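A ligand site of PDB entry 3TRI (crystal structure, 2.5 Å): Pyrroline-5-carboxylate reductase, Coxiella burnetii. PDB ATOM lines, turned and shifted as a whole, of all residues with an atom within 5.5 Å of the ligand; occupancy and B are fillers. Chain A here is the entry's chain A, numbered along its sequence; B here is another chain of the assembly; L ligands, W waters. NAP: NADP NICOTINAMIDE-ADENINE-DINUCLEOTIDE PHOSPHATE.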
ATOM      1  N   ILE A   9      -8.752 -11.190 -13.079  1.00  0.00           N
ATOM      2  CA  ILE A   9      -8.188  -9.870 -13.285  1.00  0.00           C
ATOM      3  C   ILE A   9      -6.688 -10.033 -13.434  1.00  0.00           C
ATOM      4  O   ILE A   9      -6.006 -10.417 -12.484  1.00  0.00           O
ATOM      5  CB  ILE A   9      -8.506  -8.931 -12.106  1.00  0.00           C
ATOM      6  CG1 ILE A   9     -10.019  -8.897 -11.847  1.00  0.00           C
ATOM      7  CG2 ILE A   9      -7.981  -7.525 -12.386  1.00  0.00           C
ATOM      8  CD1 ILE A   9     -10.836  -8.572 -13.075  1.00  0.00           C
ATOM      9  N   GLY A  10      -6.192  -9.748 -14.628  1.00  0.00           N
ATOM     10  CA  GLY A  10      -4.812 -10.041 -14.950  1.00  0.00           C
ATOM     11  C   GLY A  10      -4.753 -11.419 -15.572  1.00  0.00           C
ATOM     12  O   GLY A  10      -5.481 -12.327 -15.158  1.00  0.00           O
ATOM     13  N   GLY A  11      -3.917 -11.573 -16.583  1.00  0.00           N
ATOM     14  CA  GLY A  11      -3.788 -12.840 -17.275  1.00  0.00           C
ATOM     15  C   GLY A  11      -2.340 -13.252 -17.403  1.00  0.00           C
ATOM     16  O   GLY A  11      -1.884 -13.603 -18.489  1.00  0.00           O
ATOM     17  N   GLY A  12      -1.613 -13.204 -16.284  1.00  0.00           N
ATOM     18  CA  GLY A  12      -0.203 -13.538 -16.269  1.00  0.00           C
ATOM     19  C   GLY A  12       0.051 -15.033 -16.175  1.00  0.00           C
ATOM     20  O   GLY A  12      -0.692 -15.835 -16.745  1.00  0.00           O
ATOM     21  N   ASN A  13       1.093 -15.407 -15.442  1.00  0.00           N
ATOM     22  CA  ASN A  13       1.447 -16.814 -15.263  1.00  0.00           C
ATOM     23  C   ASN A  13       0.445 -17.583 -14.414  1.00  0.00           C
ATOM     24  O   ASN A  13      -0.075 -18.615 -14.839  1.00  0.00           O
ATOM     25  CB  ASN A  13       2.854 -16.935 -14.678  1.00  0.00           C
ATOM     26  CG  ASN A  13       3.936 -16.447 -15.633  1.00  0.00           C
ATOM     27  OD1 ASN A  13       3.881 -16.722 -16.827  1.00  0.00           O
ATOM     28  ND2 ASN A  13       4.914 -15.726 -15.104  1.00  0.00           N
ATOM     29  N   MET A  14       0.160 -17.070 -13.224  1.00  0.00           N
ATOM     30  CA  MET A  14      -0.776 -17.737 -12.326  1.00  0.00           C
ATOM     31  C   MET A  14      -2.161 -17.854 -12.940  1.00  0.00           C
ATOM     32  O   MET A  14      -2.782 -18.923 -12.885  1.00  0.00           O
ATOM     33  CB  MET A  14      -0.850 -16.986 -10.984  1.00  0.00           C
ATOM     34  CG  MET A  14      -1.241 -17.874  -9.812  1.00  0.00           C
ATOM     35  SD  MET A  14      -0.170 -19.506  -9.705  1.00  0.00           S
ATOM     36  CE  MET A  14      -1.365 -20.721 -10.632  1.00  0.00           C
ATOM     37  N   ALA A  15      -2.655 -16.771 -13.533  1.00  0.00           N
ATOM     38  CA  ALA A  15      -3.957 -16.797 -14.182  1.00  0.00           C
ATOM     39  C   ALA A  15      -3.974 -17.830 -15.306  1.00  0.00           C
ATOM     40  O   ALA A  15      -4.888 -18.640 -15.396  1.00  0.00           O
ATOM     41  CB  ALA A  15      -4.310 -15.425 -14.724  1.00  0.00           C
ATOM     42  N   THR A  35      -8.881 -10.905 -18.059  1.00  0.00           N
ATOM     43  CA  THR A  35      -8.554  -9.539 -18.410  1.00  0.00           C
ATOM     44  C   THR A  35      -7.073  -9.320 -18.159  1.00  0.00           C
ATOM     45  O   THR A  35      -6.451 -10.061 -17.401  1.00  0.00           O
ATOM     46  CB  THR A  35      -9.355  -8.522 -17.561  1.00  0.00           C
ATOM     47  OG1 THR A  35      -8.702  -8.338 -16.297  1.00  0.00           O
ATOM     48  CG2 THR A  35     -10.779  -9.015 -17.347  1.00  0.00           C
ATOM     49  N   ASN A  36      -6.496  -8.324 -18.815  1.00  0.00           N
ATOM     50  CA  ASN A  36      -5.082  -7.999 -18.624  1.00  0.00           C
ATOM     51  C   ASN A  36      -4.788  -6.622 -19.201  1.00  0.00           C
ATOM     52  O   ASN A  36      -5.272  -6.280 -20.281  1.00  0.00           O
ATOM     53  CB  ASN A  36      -4.196  -9.065 -19.268  1.00  0.00           C
ATOM     54  CG  ASN A  36      -2.745  -8.934 -18.866  1.00  0.00           C
ATOM     55  OD1 ASN A  36      -2.339  -9.416 -17.810  1.00  0.00           O
ATOM     56  ND2 ASN A  36      -1.948  -8.292 -19.716  1.00  0.00           N
ATOM     57  N   ARG A  37      -4.002  -5.840 -18.481  1.00  0.00           N
ATOM     58  CA  ARG A  37      -3.733  -4.466 -18.906  1.00  0.00           C
ATOM     59  C   ARG A  37      -3.149  -4.432 -20.323  1.00  0.00           C
ATOM     60  O   ARG A  37      -3.532  -3.582 -21.129  1.00  0.00           O
ATOM     61  CB  ARG A  37      -2.822  -3.748 -17.917  1.00  0.00           C
ATOM     62  CG  ARG A  37      -1.401  -4.254 -17.914  1.00  0.00           C
ATOM     63  CD  ARG A  37      -0.422  -3.102 -17.758  1.00  0.00           C
ATOM     64  NE  ARG A  37      -0.430  -2.529 -16.415  1.00  0.00           N
ATOM     65  CZ  ARG A  37       0.489  -2.797 -15.491  1.00  0.00           C
ATOM     66  NH1 ARG A  37       1.489  -3.624 -15.770  1.00  0.00           N
ATOM     67  NH2 ARG A  37       0.407  -2.230 -14.291  1.00  0.00           N
ATOM     68  N   SER A  38      -2.234  -5.347 -20.628  1.00  0.00           N
ATOM     69  CA  SER A  38      -1.667  -5.421 -21.966  1.00  0.00           C
ATOM     70  C   SER A  38      -2.345  -6.504 -22.805  1.00  0.00           C
ATOM     71  O   SER A  38      -2.854  -7.492 -22.276  1.00  0.00           O
ATOM     72  CB  SER A  38      -0.149  -5.621 -21.931  1.00  0.00           C
ATOM     73  OG  SER A  38       0.190  -6.979 -21.759  1.00  0.00           O
ATOM     74  N   LYS A  41      -0.808 -10.906 -23.948  1.00  0.00           N
ATOM     75  CA  LYS A  41      -1.024 -12.067 -23.096  1.00  0.00           C
ATOM     76  C   LYS A  41      -2.432 -12.654 -23.274  1.00  0.00           C
ATOM     77  O   LYS A  41      -2.630 -13.847 -23.074  1.00  0.00           O
ATOM     78  CB  LYS A  41      -0.765 -11.712 -21.632  1.00  0.00           C
ATOM     79  CG  LYS A  41       0.693 -11.400 -21.340  1.00  0.00           C
ATOM     80  CD  LYS A  41       0.920 -11.003 -19.891  1.00  0.00           C
ATOM     81  CE  LYS A  41       2.384 -10.618 -19.679  1.00  0.00           C
ATOM     82  NZ  LYS A  41       2.672 -10.212 -18.277  1.00  0.00           N
ATOM     83  N   ASN A  57     -10.861  -4.300 -17.145  1.00  0.00           N
ATOM     84  CA  ASN A  57     -11.184  -5.006 -15.913  1.00  0.00           C
ATOM     85  C   ASN A  57     -12.665  -4.973 -15.539  1.00  0.00           C
ATOM     86  O   ASN A  57     -13.231  -5.973 -15.115  1.00  0.00           O
ATOM     87  CB  ASN A  57     -10.348  -4.484 -14.747  1.00  0.00           C
ATOM     88  CG  ASN A  57      -8.865  -4.799 -14.893  1.00  0.00           C
ATOM     89  OD1 ASN A  57      -8.443  -5.368 -15.903  1.00  0.00           O
ATOM     90  ND2 ASN A  57      -8.084  -4.433 -13.890  1.00  0.00           N
ATOM     91  N   LEU A  69      -8.398 -12.229  -8.425  1.00  0.00           N
ATOM     92  CA  LEU A  69      -7.383 -11.199  -8.595  1.00  0.00           C
ATOM     93  C   LEU A  69      -6.016 -11.828  -8.820  1.00  0.00           C
ATOM     94  O   LEU A  69      -5.402 -12.358  -7.888  1.00  0.00           O
ATOM     95  CB  LEU A  69      -7.343 -10.272  -7.379  1.00  0.00           C
ATOM     96  CG  LEU A  69      -8.677  -9.695  -6.922  1.00  0.00           C
ATOM     97  CD1 LEU A  69      -8.488  -8.749  -5.746  1.00  0.00           C
ATOM     98  CD2 LEU A  69      -9.394  -8.984  -8.069  1.00  0.00           C
ATOM     99  N   ALA A  70      -5.549 -11.776 -10.063  1.00  0.00           N
ATOM    100  CA  ALA A  70      -4.301 -12.416 -10.457  1.00  0.00           C
ATOM    101  C   ALA A  70      -3.277 -11.398 -10.954  1.00  0.00           C
ATOM    102  O   ALA A  70      -2.544 -11.661 -11.904  1.00  0.00           O
ATOM    103  CB  ALA A  70      -4.561 -13.479 -11.513  1.00  0.00           C
ATOM    104  N   VAL A  71      -3.247 -10.244 -10.320  1.00  0.00           N
ATOM    105  CA  VAL A  71      -2.257  -9.234 -10.646  1.00  0.00           C
ATOM    106  C   VAL A  71      -1.181  -9.244  -9.572  1.00  0.00           C
ATOM    107  O   VAL A  71      -1.350  -9.904  -8.537  1.00  0.00           O
ATOM    108  CB  VAL A  71      -2.873  -7.817 -10.752  1.00  0.00           C
ATOM    109  CG1 VAL A  71      -3.900  -7.769 -11.874  1.00  0.00           C
ATOM    110  CG2 VAL A  71      -3.501  -7.399  -9.428  1.00  0.00           C
ATOM    111  N   LYS A  72      -0.076  -8.546  -9.807  1.00  0.00           N
ATOM    112  CA  LYS A  72       0.982  -8.414  -8.817  1.00  0.00           C
ATOM    113  C   LYS A  72       0.371  -7.905  -7.521  1.00  0.00           C
ATOM    114  O   LYS A  72      -0.676  -7.256  -7.552  1.00  0.00           O
ATOM    115  CB  LYS A  72       2.068  -7.454  -9.300  1.00  0.00           C
ATOM    116  CG  LYS A  72       2.752  -7.842 -10.594  1.00  0.00           C
ATOM    117  CD  LYS A  72       3.729  -8.999 -10.400  1.00  0.00           C
ATOM    118  CE  LYS A  72       4.633  -9.149 -11.620  1.00  0.00           C
ATOM    119  NZ  LYS A  72       5.505 -10.348 -11.533  1.00  0.00           N
ATOM    120  N   PRO A  73       1.009  -8.189  -6.389  1.00  0.00           N
ATOM    121  CA  PRO A  73       0.493  -7.753  -5.081  1.00  0.00           C
ATOM    122  C   PRO A  73       0.364  -6.234  -5.005  1.00  0.00           C
ATOM    123  O   PRO A  73      -0.567  -5.735  -4.376  1.00  0.00           O
ATOM    124  CB  PRO A  73       1.560  -8.249  -4.097  1.00  0.00           C
ATOM    125  CG  PRO A  73       2.200  -9.400  -4.785  1.00  0.00           C
ATOM    126  CD  PRO A  73       2.216  -9.024  -6.237  1.00  0.00           C
ATOM    127  N   GLN A  75      -0.512  -4.328  -7.199  1.00  0.00           N
ATOM    128  CA  GLN A  75      -1.492  -3.914  -8.198  1.00  0.00           C
ATOM    129  C   GLN A  75      -2.892  -4.310  -7.747  1.00  0.00           C
ATOM    130  O   GLN A  75      -3.875  -4.088  -8.464  1.00  0.00           O
ATOM    131  CB  GLN A  75      -1.178  -4.545  -9.552  1.00  0.00           C
ATOM    132  CG  GLN A  75       0.189  -4.206 -10.099  1.00  0.00           C
ATOM    133  CD  GLN A  75       0.595  -5.115 -11.239  1.00  0.00           C
ATOM    134  OE1 GLN A  75       0.030  -6.200 -11.421  1.00  0.00           O
ATOM    135  NE2 GLN A  75       1.573  -4.685 -12.034  1.00  0.00           N
ATOM    136  N   ILE A  76      -2.976  -4.907  -6.562  1.00  0.00           N
ATOM    137  CA  ILE A  76      -4.237  -5.372  -6.012  1.00  0.00           C
ATOM    138  C   ILE A  76      -5.122  -4.206  -5.563  1.00  0.00           C
ATOM    139  O   ILE A  76      -6.322  -4.202  -5.795  1.00  0.00           O
ATOM    140  CB  ILE A  76      -4.001  -6.326  -4.815  1.00  0.00           C
ATOM    141  CG1 ILE A  76      -3.382  -7.633  -5.299  1.00  0.00           C
ATOM    142  CG2 ILE A  76      -5.291  -6.599  -4.064  1.00  0.00           C
ATOM    143  CD1 ILE A  76      -4.300  -8.468  -6.177  1.00  0.00           C
ATOM    144  N   MET A  78      -5.327  -0.924  -6.543  1.00  0.00           N
ATOM    145  CA  MET A  78      -5.979  -0.206  -7.639  1.00  0.00           C
ATOM    146  C   MET A  78      -7.066  -1.056  -8.273  1.00  0.00           C
ATOM    147  O   MET A  78      -8.176  -0.586  -8.504  1.00  0.00           O
ATOM    148  CB  MET A  78      -4.970   0.237  -8.691  1.00  0.00           C
ATOM    149  CG  MET A  78      -4.154  -0.892  -9.320  1.00  0.00           C
ATOM    150  SD  MET A  78      -3.438  -0.364 -11.062  1.00  0.00           S
ATOM    151  CE  MET A  78      -1.991  -1.665 -11.241  1.00  0.00           C
ATOM    152  N   VAL A  79      -6.742  -2.316  -8.545  1.00  0.00           N
ATOM    153  CA  VAL A  79      -7.704  -3.248  -9.111  1.00  0.00           C
ATOM    154  C   VAL A  79      -8.968  -3.324  -8.258  1.00  0.00           C
ATOM    155  O   VAL A  79     -10.074  -3.398  -8.776  1.00  0.00           O
ATOM    156  CB  VAL A  79      -7.077  -4.652  -9.288  1.00  0.00           C
ATOM    157  CG1 VAL A  79      -8.152  -5.724  -9.327  1.00  0.00           C
ATOM    158  CG2 VAL A  79      -6.218  -4.694 -10.543  1.00  0.00           C
ATOM    159  N   GLU A  82     -10.756   0.064  -8.582  1.00  0.00           N
ATOM    160  CA  GLU A  82     -11.303   0.078  -9.933  1.00  0.00           C
ATOM    161  C   GLU A  82     -12.621  -0.687 -10.023  1.00  0.00           C
ATOM    162  O   GLU A  82     -13.474  -0.364 -10.844  1.00  0.00           O
ATOM    163  CB  GLU A  82     -10.271  -0.516 -10.912  1.00  0.00           C
ATOM    164  CG  GLU A  82     -10.762  -0.654 -12.345  1.00  0.00           C
ATOM    165  CD  GLU A  82      -9.673  -1.189 -13.275  1.00  0.00           C
ATOM    166  OE1 GLU A  82      -8.576  -1.531 -12.787  1.00  0.00           O
ATOM    167  OE2 GLU A  82      -9.918  -1.258 -14.504  1.00  0.00           O
ATOM    168  N   LEU A  97      -5.115 -13.918  -5.098  1.00  0.00           N
ATOM    169  CA  LEU A  97      -3.993 -14.843  -5.187  1.00  0.00           C
ATOM    170  C   LEU A  97      -2.732 -14.175  -4.674  1.00  0.00           C
ATOM    171  O   LEU A  97      -1.715 -14.828  -4.458  1.00  0.00           O
ATOM    172  CB  LEU A  97      -3.774 -15.267  -6.637  1.00  0.00           C
ATOM    173  CG  LEU A  97      -4.986 -15.742  -7.427  1.00  0.00           C
ATOM    174  CD1 LEU A  97      -4.583 -16.096  -8.844  1.00  0.00           C
ATOM    175  CD2 LEU A  97      -5.642 -16.912  -6.731  1.00  0.00           C
ATOM    176  N   ALA A  98      -2.808 -12.863  -4.469  1.00  0.00           N
ATOM    177  CA  ALA A  98      -1.626 -12.066  -4.183  1.00  0.00           C
ATOM    178  C   ALA A  98      -0.931 -12.474  -2.898  1.00  0.00           C
ATOM    179  O   ALA A  98      -1.573 -12.622  -1.857  1.00  0.00           O
ATOM    180  CB  ALA A  98      -1.969 -10.584  -4.152  1.00  0.00           C
ATOM    181  N   VAL A  99       0.383 -12.642  -2.973  1.00  0.00           N
ATOM    182  CA  VAL A  99       1.189 -12.844  -1.785  1.00  0.00           C
ATOM    183  C   VAL A  99       1.334 -11.494  -1.077  1.00  0.00           C
ATOM    184  O   VAL A  99       1.458 -10.461  -1.726  1.00  0.00           O
ATOM    185  CB  VAL A  99       2.592 -13.385  -2.133  1.00  0.00           C
ATOM    186  CG1 VAL A  99       3.435 -13.559  -0.880  1.00  0.00           C
ATOM    187  CG2 VAL A  99       2.471 -14.709  -2.879  1.00  0.00           C
ATOM    188  N   MET A 120      -3.637 -19.479  -2.231  1.00  0.00           N
ATOM    189  CA  MET A 120      -2.215 -19.550  -2.517  1.00  0.00           C
ATOM    190  C   MET A 120      -1.931 -20.774  -3.382  1.00  0.00           C
ATOM    191  O   MET A 120      -1.512 -21.814  -2.879  1.00  0.00           O
ATOM    192  CB  MET A 120      -1.413 -19.614  -1.224  1.00  0.00           C
ATOM    193  CG  MET A 120       0.087 -19.474  -1.425  1.00  0.00           C
ATOM    194  SD  MET A 120       0.515 -17.992  -2.628  1.00  0.00           S
ATOM    195  CE  MET A 120      -0.584 -16.597  -1.804  1.00  0.00           C
ATOM    196  N   PRO A 121      -2.157 -20.640  -4.694  1.00  0.00           N
ATOM    197  CA  PRO A 121      -2.013 -21.731  -5.658  1.00  0.00           C
ATOM    198  C   PRO A 121      -0.584 -21.827  -6.175  1.00  0.00           C
ATOM    199  O   PRO A 121       0.286 -21.079  -5.730  1.00  0.00           O
ATOM    200  CB  PRO A 121      -2.930 -21.280  -6.792  1.00  0.00           C
ATOM    201  CG  PRO A 121      -2.769 -19.793  -6.802  1.00  0.00           C
ATOM    202  CD  PRO A 121      -2.567 -19.381  -5.360  1.00  0.00           C
ATOM    203  N   ASN A 122      -0.358 -22.732  -7.107  1.00  0.00           N
ATOM    204  CA  ASN A 122       0.924 -22.834  -7.787  1.00  0.00           C
ATOM    205  C   ASN A 122       0.754 -23.243  -9.245  1.00  0.00           C
ATOM    206  O   ASN A 122      -0.320 -23.652  -9.661  1.00  0.00           O
ATOM    207  CB  ASN A 122       1.885 -23.762  -7.033  1.00  0.00           C
ATOM    208  CG  ASN A 122       1.384 -25.200  -6.947  1.00  0.00           C
ATOM    209  OD1 ASN A 122       0.428 -25.590  -7.626  1.00  0.00           O
ATOM    210  ND2 ASN A 122       2.044 -26.001  -6.130  1.00  0.00           N
ATOM    211  N   THR A 123       1.822 -23.101 -10.030  1.00  0.00           N
ATOM    212  CA  THR A 123       1.749 -23.306 -11.474  1.00  0.00           C
ATOM    213  C   THR A 123       1.303 -24.689 -11.947  1.00  0.00           C
ATOM    214  O   THR A 123       0.689 -24.804 -13.008  1.00  0.00           O
ATOM    215  CB  THR A 123       3.077 -22.928 -12.147  1.00  0.00           C
ATOM    216  OG1 THR A 123       4.160 -23.564 -11.462  1.00  0.00           O
ATOM    217  CG2 THR A 123       3.282 -21.423 -12.097  1.00  0.00           C
ATOM    218  N   GLY A 175       3.789 -22.452  -2.916  1.00  0.00           N
ATOM    219  CA  GLY A 175       3.673 -21.351  -3.847  1.00  0.00           C
ATOM    220  C   GLY A 175       4.927 -21.231  -4.690  1.00  0.00           C
ATOM    221  O   GLY A 175       4.872 -21.270  -5.912  1.00  0.00           O
ATOM    222  N   PHE B 230       7.927 -19.029 -14.907  1.00  0.00           N
ATOM    223  CA  PHE B 230       6.501 -18.875 -14.626  1.00  0.00           C
ATOM    224  C   PHE B 230       6.259 -18.687 -13.127  1.00  0.00           C
ATOM    225  O   PHE B 230       5.289 -18.048 -12.713  1.00  0.00           O
ATOM    226  CB  PHE B 230       5.707 -20.084 -15.134  1.00  0.00           C
ATOM    227  CG  PHE B 230       5.752 -20.269 -16.627  1.00  0.00           C
ATOM    228  CD1 PHE B 230       6.275 -19.287 -17.433  1.00  0.00           C
ATOM    229  CD2 PHE B 230       5.262 -21.429 -17.214  1.00  0.00           C
ATOM    230  CE1 PHE B 230       6.318 -19.448 -18.812  1.00  0.00           C
ATOM    231  CE2 PHE B 230       5.305 -21.590 -18.593  1.00  0.00           C
ATOM    232  CZ  PHE B 230       5.832 -20.604 -19.386  1.00  0.00           C
ATOM    233  N   VAL B 231       7.147 -19.250 -12.315  1.00  0.00           N
ATOM    234  CA  VAL B 231       6.994 -19.187 -10.869  1.00  0.00           C
ATOM    235  C   VAL B 231       7.640 -17.918 -10.310  1.00  0.00           C
ATOM    236  O   VAL B 231       7.181 -17.370  -9.307  1.00  0.00           O
ATOM    237  CB  VAL B 231       7.633 -20.428 -10.193  1.00  0.00           C
ATOM    238  CG1 VAL B 231       7.418 -20.368  -8.679  1.00  0.00           C
ATOM    239  CG2 VAL B 231       7.056 -21.712 -10.779  1.00  0.00           C
ATOM    240  N   THR B 232       8.696 -17.476 -10.974  1.00  0.00           N
ATOM    241  CA  THR B 232       9.502 -16.357 -10.491  1.00  0.00           C
ATOM    242  C   THR B 232       9.073 -15.027 -11.085  1.00  0.00           C
ATOM    243  O   THR B 232       9.030 -14.848 -12.301  1.00  0.00           O
ATOM    244  CB  THR B 232      10.999 -16.559 -10.802  1.00  0.00           C
ATOM    245  OG1 THR B 232      11.373 -17.903 -10.467  1.00  0.00           O
ATOM    246  CG2 THR B 232      11.854 -15.582 -10.013  1.00  0.00           C
ATOM    247  N   SER B 233       8.735 -14.080 -10.218  1.00  0.00           N
ATOM    248  CA  SER B 233       8.522 -12.703 -10.625  1.00  0.00           C
ATOM    249  C   SER B 233       9.766 -11.910 -10.252  1.00  0.00           C
ATOM    250  O   SER B 233      10.306 -12.076  -9.154  1.00  0.00           O
ATOM    251  CB  SER B 233       7.290 -12.114  -9.950  1.00  0.00           C
ATOM    252  OG  SER B 233       7.507 -11.950  -8.563  1.00  0.00           O
HETATM  253  PA  NAP L   1       2.453 -11.924 -13.809  1.00  0.00           P
HETATM  254  O1A NAP L   1       3.766 -11.271 -13.594  1.00  0.00           O
HETATM  255  O2A NAP L   1       2.569 -13.032 -14.776  1.00  0.00           O
HETATM  256  O5B NAP L   1       1.401 -10.806 -14.293  1.00  0.00           O
HETATM  257  C5B NAP L   1       0.049 -10.803 -13.892  1.00  0.00           C
HETATM  258  C4B NAP L   1      -0.690  -9.955 -14.922  1.00  0.00           C
HETATM  259  O4B NAP L   1      -1.500  -8.952 -14.326  1.00  0.00           O
HETATM  260  C3B NAP L   1       0.286  -9.220 -15.830  1.00  0.00           C
HETATM  261  O3B NAP L   1       0.230  -9.809 -17.114  1.00  0.00           O
HETATM  262  C2B NAP L   1      -0.178  -7.776 -15.881  1.00  0.00           C
HETATM  263  O2B NAP L   1      -0.271  -7.309 -17.202  1.00  0.00           O
HETATM  264  C1B NAP L   1      -1.547  -7.859 -15.225  1.00  0.00           C
HETATM  265  N9A NAP L   1      -1.946  -6.578 -14.621  1.00  0.00           N
HETATM  266  C8A NAP L   1      -1.164  -5.713 -13.906  1.00  0.00           C
HETATM  267  N7A NAP L   1      -1.925  -4.653 -13.541  1.00  0.00           N
HETATM  268  C5A NAP L   1      -3.186  -4.848 -14.004  1.00  0.00           C
HETATM  269  C6A NAP L   1      -4.340  -4.090 -13.918  1.00  0.00           C
HETATM  270  N6A NAP L   1      -4.344  -2.928 -13.272  1.00  0.00           N
HETATM  271  N1A NAP L   1      -5.501  -4.549 -14.511  1.00  0.00           N
HETATM  272  C2A NAP L   1      -5.514  -5.754 -15.184  1.00  0.00           C
HETATM  273  N3A NAP L   1      -4.344  -6.496 -15.263  1.00  0.00           N
HETATM  274  C4A NAP L   1      -3.204  -6.048 -14.693  1.00  0.00           C
HETATM  275  O3  NAP L   1       1.814 -12.437 -12.427  1.00  0.00           O
HETATM  276  PN  NAP L   1       1.790 -13.861 -11.696  1.00  0.00           P
HETATM  277  O1N NAP L   1       3.164 -14.408 -11.584  1.00  0.00           O
HETATM  278  O2N NAP L   1       0.722 -14.647 -12.342  1.00  0.00           O
HETATM  279  O5D NAP L   1       1.303 -13.406 -10.241  1.00  0.00           O
HETATM  280  C5D NAP L   1      -0.046 -13.031 -10.093  1.00  0.00           C
HETATM  281  C4D NAP L   1      -0.434 -13.194  -8.637  1.00  0.00           C
HETATM  282  O4D NAP L   1      -0.426 -14.564  -8.278  1.00  0.00           O
HETATM  283  C3D NAP L   1       0.582 -12.488  -7.760  1.00  0.00           C
HETATM  284  O3D NAP L   1      -0.101 -11.697  -6.821  1.00  0.00           O
HETATM  285  C2D NAP L   1       1.340 -13.607  -7.078  1.00  0.00           C
HETATM  286  O2D NAP L   1       1.683 -13.248  -5.764  1.00  0.00           O
HETATM  287  C1D NAP L   1       0.351 -14.756  -7.110  1.00  0.00           C
HETATM  288  N1N NAP L   1       1.033 -16.064  -7.148  1.00  0.00           N
HETATM  289  C2N NAP L   1       1.816 -16.407  -8.220  1.00  0.00           C
HETATM  290  C3N NAP L   1       2.455 -17.647  -8.249  1.00  0.00           C
HETATM  291  C7N NAP L   1       3.347 -18.010  -9.392  1.00  0.00           C
HETATM  292  O7N NAP L   1       4.154 -19.164  -9.283  1.00  0.00           O
HETATM  293  N7N NAP L   1       3.355 -17.252 -10.485  1.00  0.00           N
HETATM  294  C4N NAP L   1       2.283 -18.548  -7.199  1.00  0.00           C
HETATM  295  C5N NAP L   1       1.477 -18.186  -6.121  1.00  0.00           C
HETATM  296  C6N NAP L   1       0.854 -16.950  -6.117  1.00  0.00           C
HETATM  297  P2B NAP L   1       1.064  -6.878 -17.988  1.00  0.00           P
HETATM  298  O1X NAP L   1       0.854  -7.161 -19.457  1.00  0.00           O
HETATM  299  O2X NAP L   1       2.267  -7.643 -17.492  1.00  0.00           O
HETATM  300  O3X NAP L   1       1.325  -5.410 -17.777  1.00  0.00           O
HETATM  301  O   HOH W   1      -1.578 -13.781 -13.487  1.00  0.00           O
HETATM  302  O   HOH W   2       4.207 -17.499  -4.459  1.00  0.00           O
HETATM  303  O   HOH W   3       3.983 -21.742  -8.256  1.00  0.00           O
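Gly 10 touches the ligand.
Gly 11 touches the ligand.
Gly 12 touches the ligand.
O of Ala 70 touches C5D of the ligand (3.4 Å).
Pro 73 touches the ligand (CD to O3D, 3.6 Å).
Val 79 touches the ligand (CG2 to N6A, 3.8 Å).
Leu 97 touches the ligand.
Ala 98 touches the ligand (CA to O3D, 3.1 Å).
Met 120 touches the ligand.
Pro 121 touches the ligand.
Thr 123 touches the ligand (CG2 to O7N, 3.7 Å).
Gly 175 touches the ligand (O to C4N, 3.97 Å).
CA of Val 231 of chain B touches O7N of the ligand, at 3.3 Å.
Hydrophobic or aromatic side chains within 4 Å of the ligand: Met 14, Val 71, Pro 73, Met 78, Val 79, Leu 97, Ala 98, Val 99, Met 120 and Val 231 of chain B.
The nearest printed residue that does not touch the ligand is Ile 9 (4.1 Å).
The side-chain amide nitrogen (ND2) of Asn 57 lies within hydrogen-bond range of the side-chain carboxylate (OE1) of Glu 82, 3.1 Å away.
The backbone NH (N) of Gly 10 lies within hydrogen-bond range of the backbone carbonyl oxygen (O) of Thr 35, 2.8 Å away.
The backbone NH (N) of Leu 97 sits at hydrogen-bond distance from the backbone carbonyl oxygen (O) of Leu 69 (3.2 Å).
O of Ser 38 lies within hydrogen-bond range of ND2 of Asn 36, 2.8 Å away.
OE1 of Gln 75 sits at hydrogen-bond distance from N of Lys 72 (2.8 Å).
ND2 of Asn 13 sits close to O of Phe 230 of chain B (3.4 Å).
OD1 of Asn 36 is in hydrogen-bond range of N of Gly 11, at 2.9 Å.
The side-chain hydroxyl (OG1) of Thr 35 is in hydrogen-bond range of the side-chain amide oxygen (OD1) of Asn 57, at 3.0 Å.
Water W1 lies within hydrogen-bond range of O2N of the ligand, O of Ala 70, N of Gly 12 and N of Ala 15.
Water W3 lies within hydrogen-bond range of the backbone carbonyl oxygen of Gly 175 (2.6 Å), an oxygen (O7N) of the ligand (2.8 Å) and the backbone NH of Thr 123 (3.1 Å).
The backbone NH (N) of Met 14 is in hydrogen-bond range of an oxygen (O2N) of the ligand (2.6 Å).
The backbone NH (N) of Arg 37 lies within hydrogen-bond range of a nitrogen (N3A) of the ligand (3.3 Å).
OD1 of Asn 36 is in hydrogen-bond range of O3B of the ligand, at 2.7 Å.
The backbone NH of Asn 13 is in hydrogen-bond range of an oxygen (O2A) of the ligand (2.9 Å).
The side-chain amide oxygen (OE1) of Gln 75 sits close to a nitrogen (N7A) of the ligand, at 3.3 Å.
N of Val 99 sits at hydrogen-bond distance from O2D of the ligand (3.1 Å).
An oxygen (O3X) of the ligand lies within salt-bridge range of the guanidinium group (NH1) of Arg 37 (2.7 Å).
An oxygen (O1X) of the ligand sits at hydrogen-bond distance from the side-chain hydroxyl (OG) of Ser 38 (2.4 Å).
The backbone carbonyl oxygen of Phe 230 of chain B sits at hydrogen-bond distance from a nitrogen (N7N) of the ligand.
The side-chain sulfur (SD) of Met 78 lies close to a nitrogen (N6A) of the ligand (3.5 Å).
The side-chain amino group (NZ) of Lys 41 lies within salt-bridge range of an oxygen (O2X) of the ligand (2.7 Å).
An oxygen (O1A) of the ligand is in salt-bridge range of the side-chain amino group (NZ) of Lys 72 (2.9 Å).
N1A of the ligand lies within hydrogen-bond range of ND2 of Asn 57 (2.7 Å).
O of Val 71 lies within hydrogen-bond range of O3D of the ligand, at 2.8 Å.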
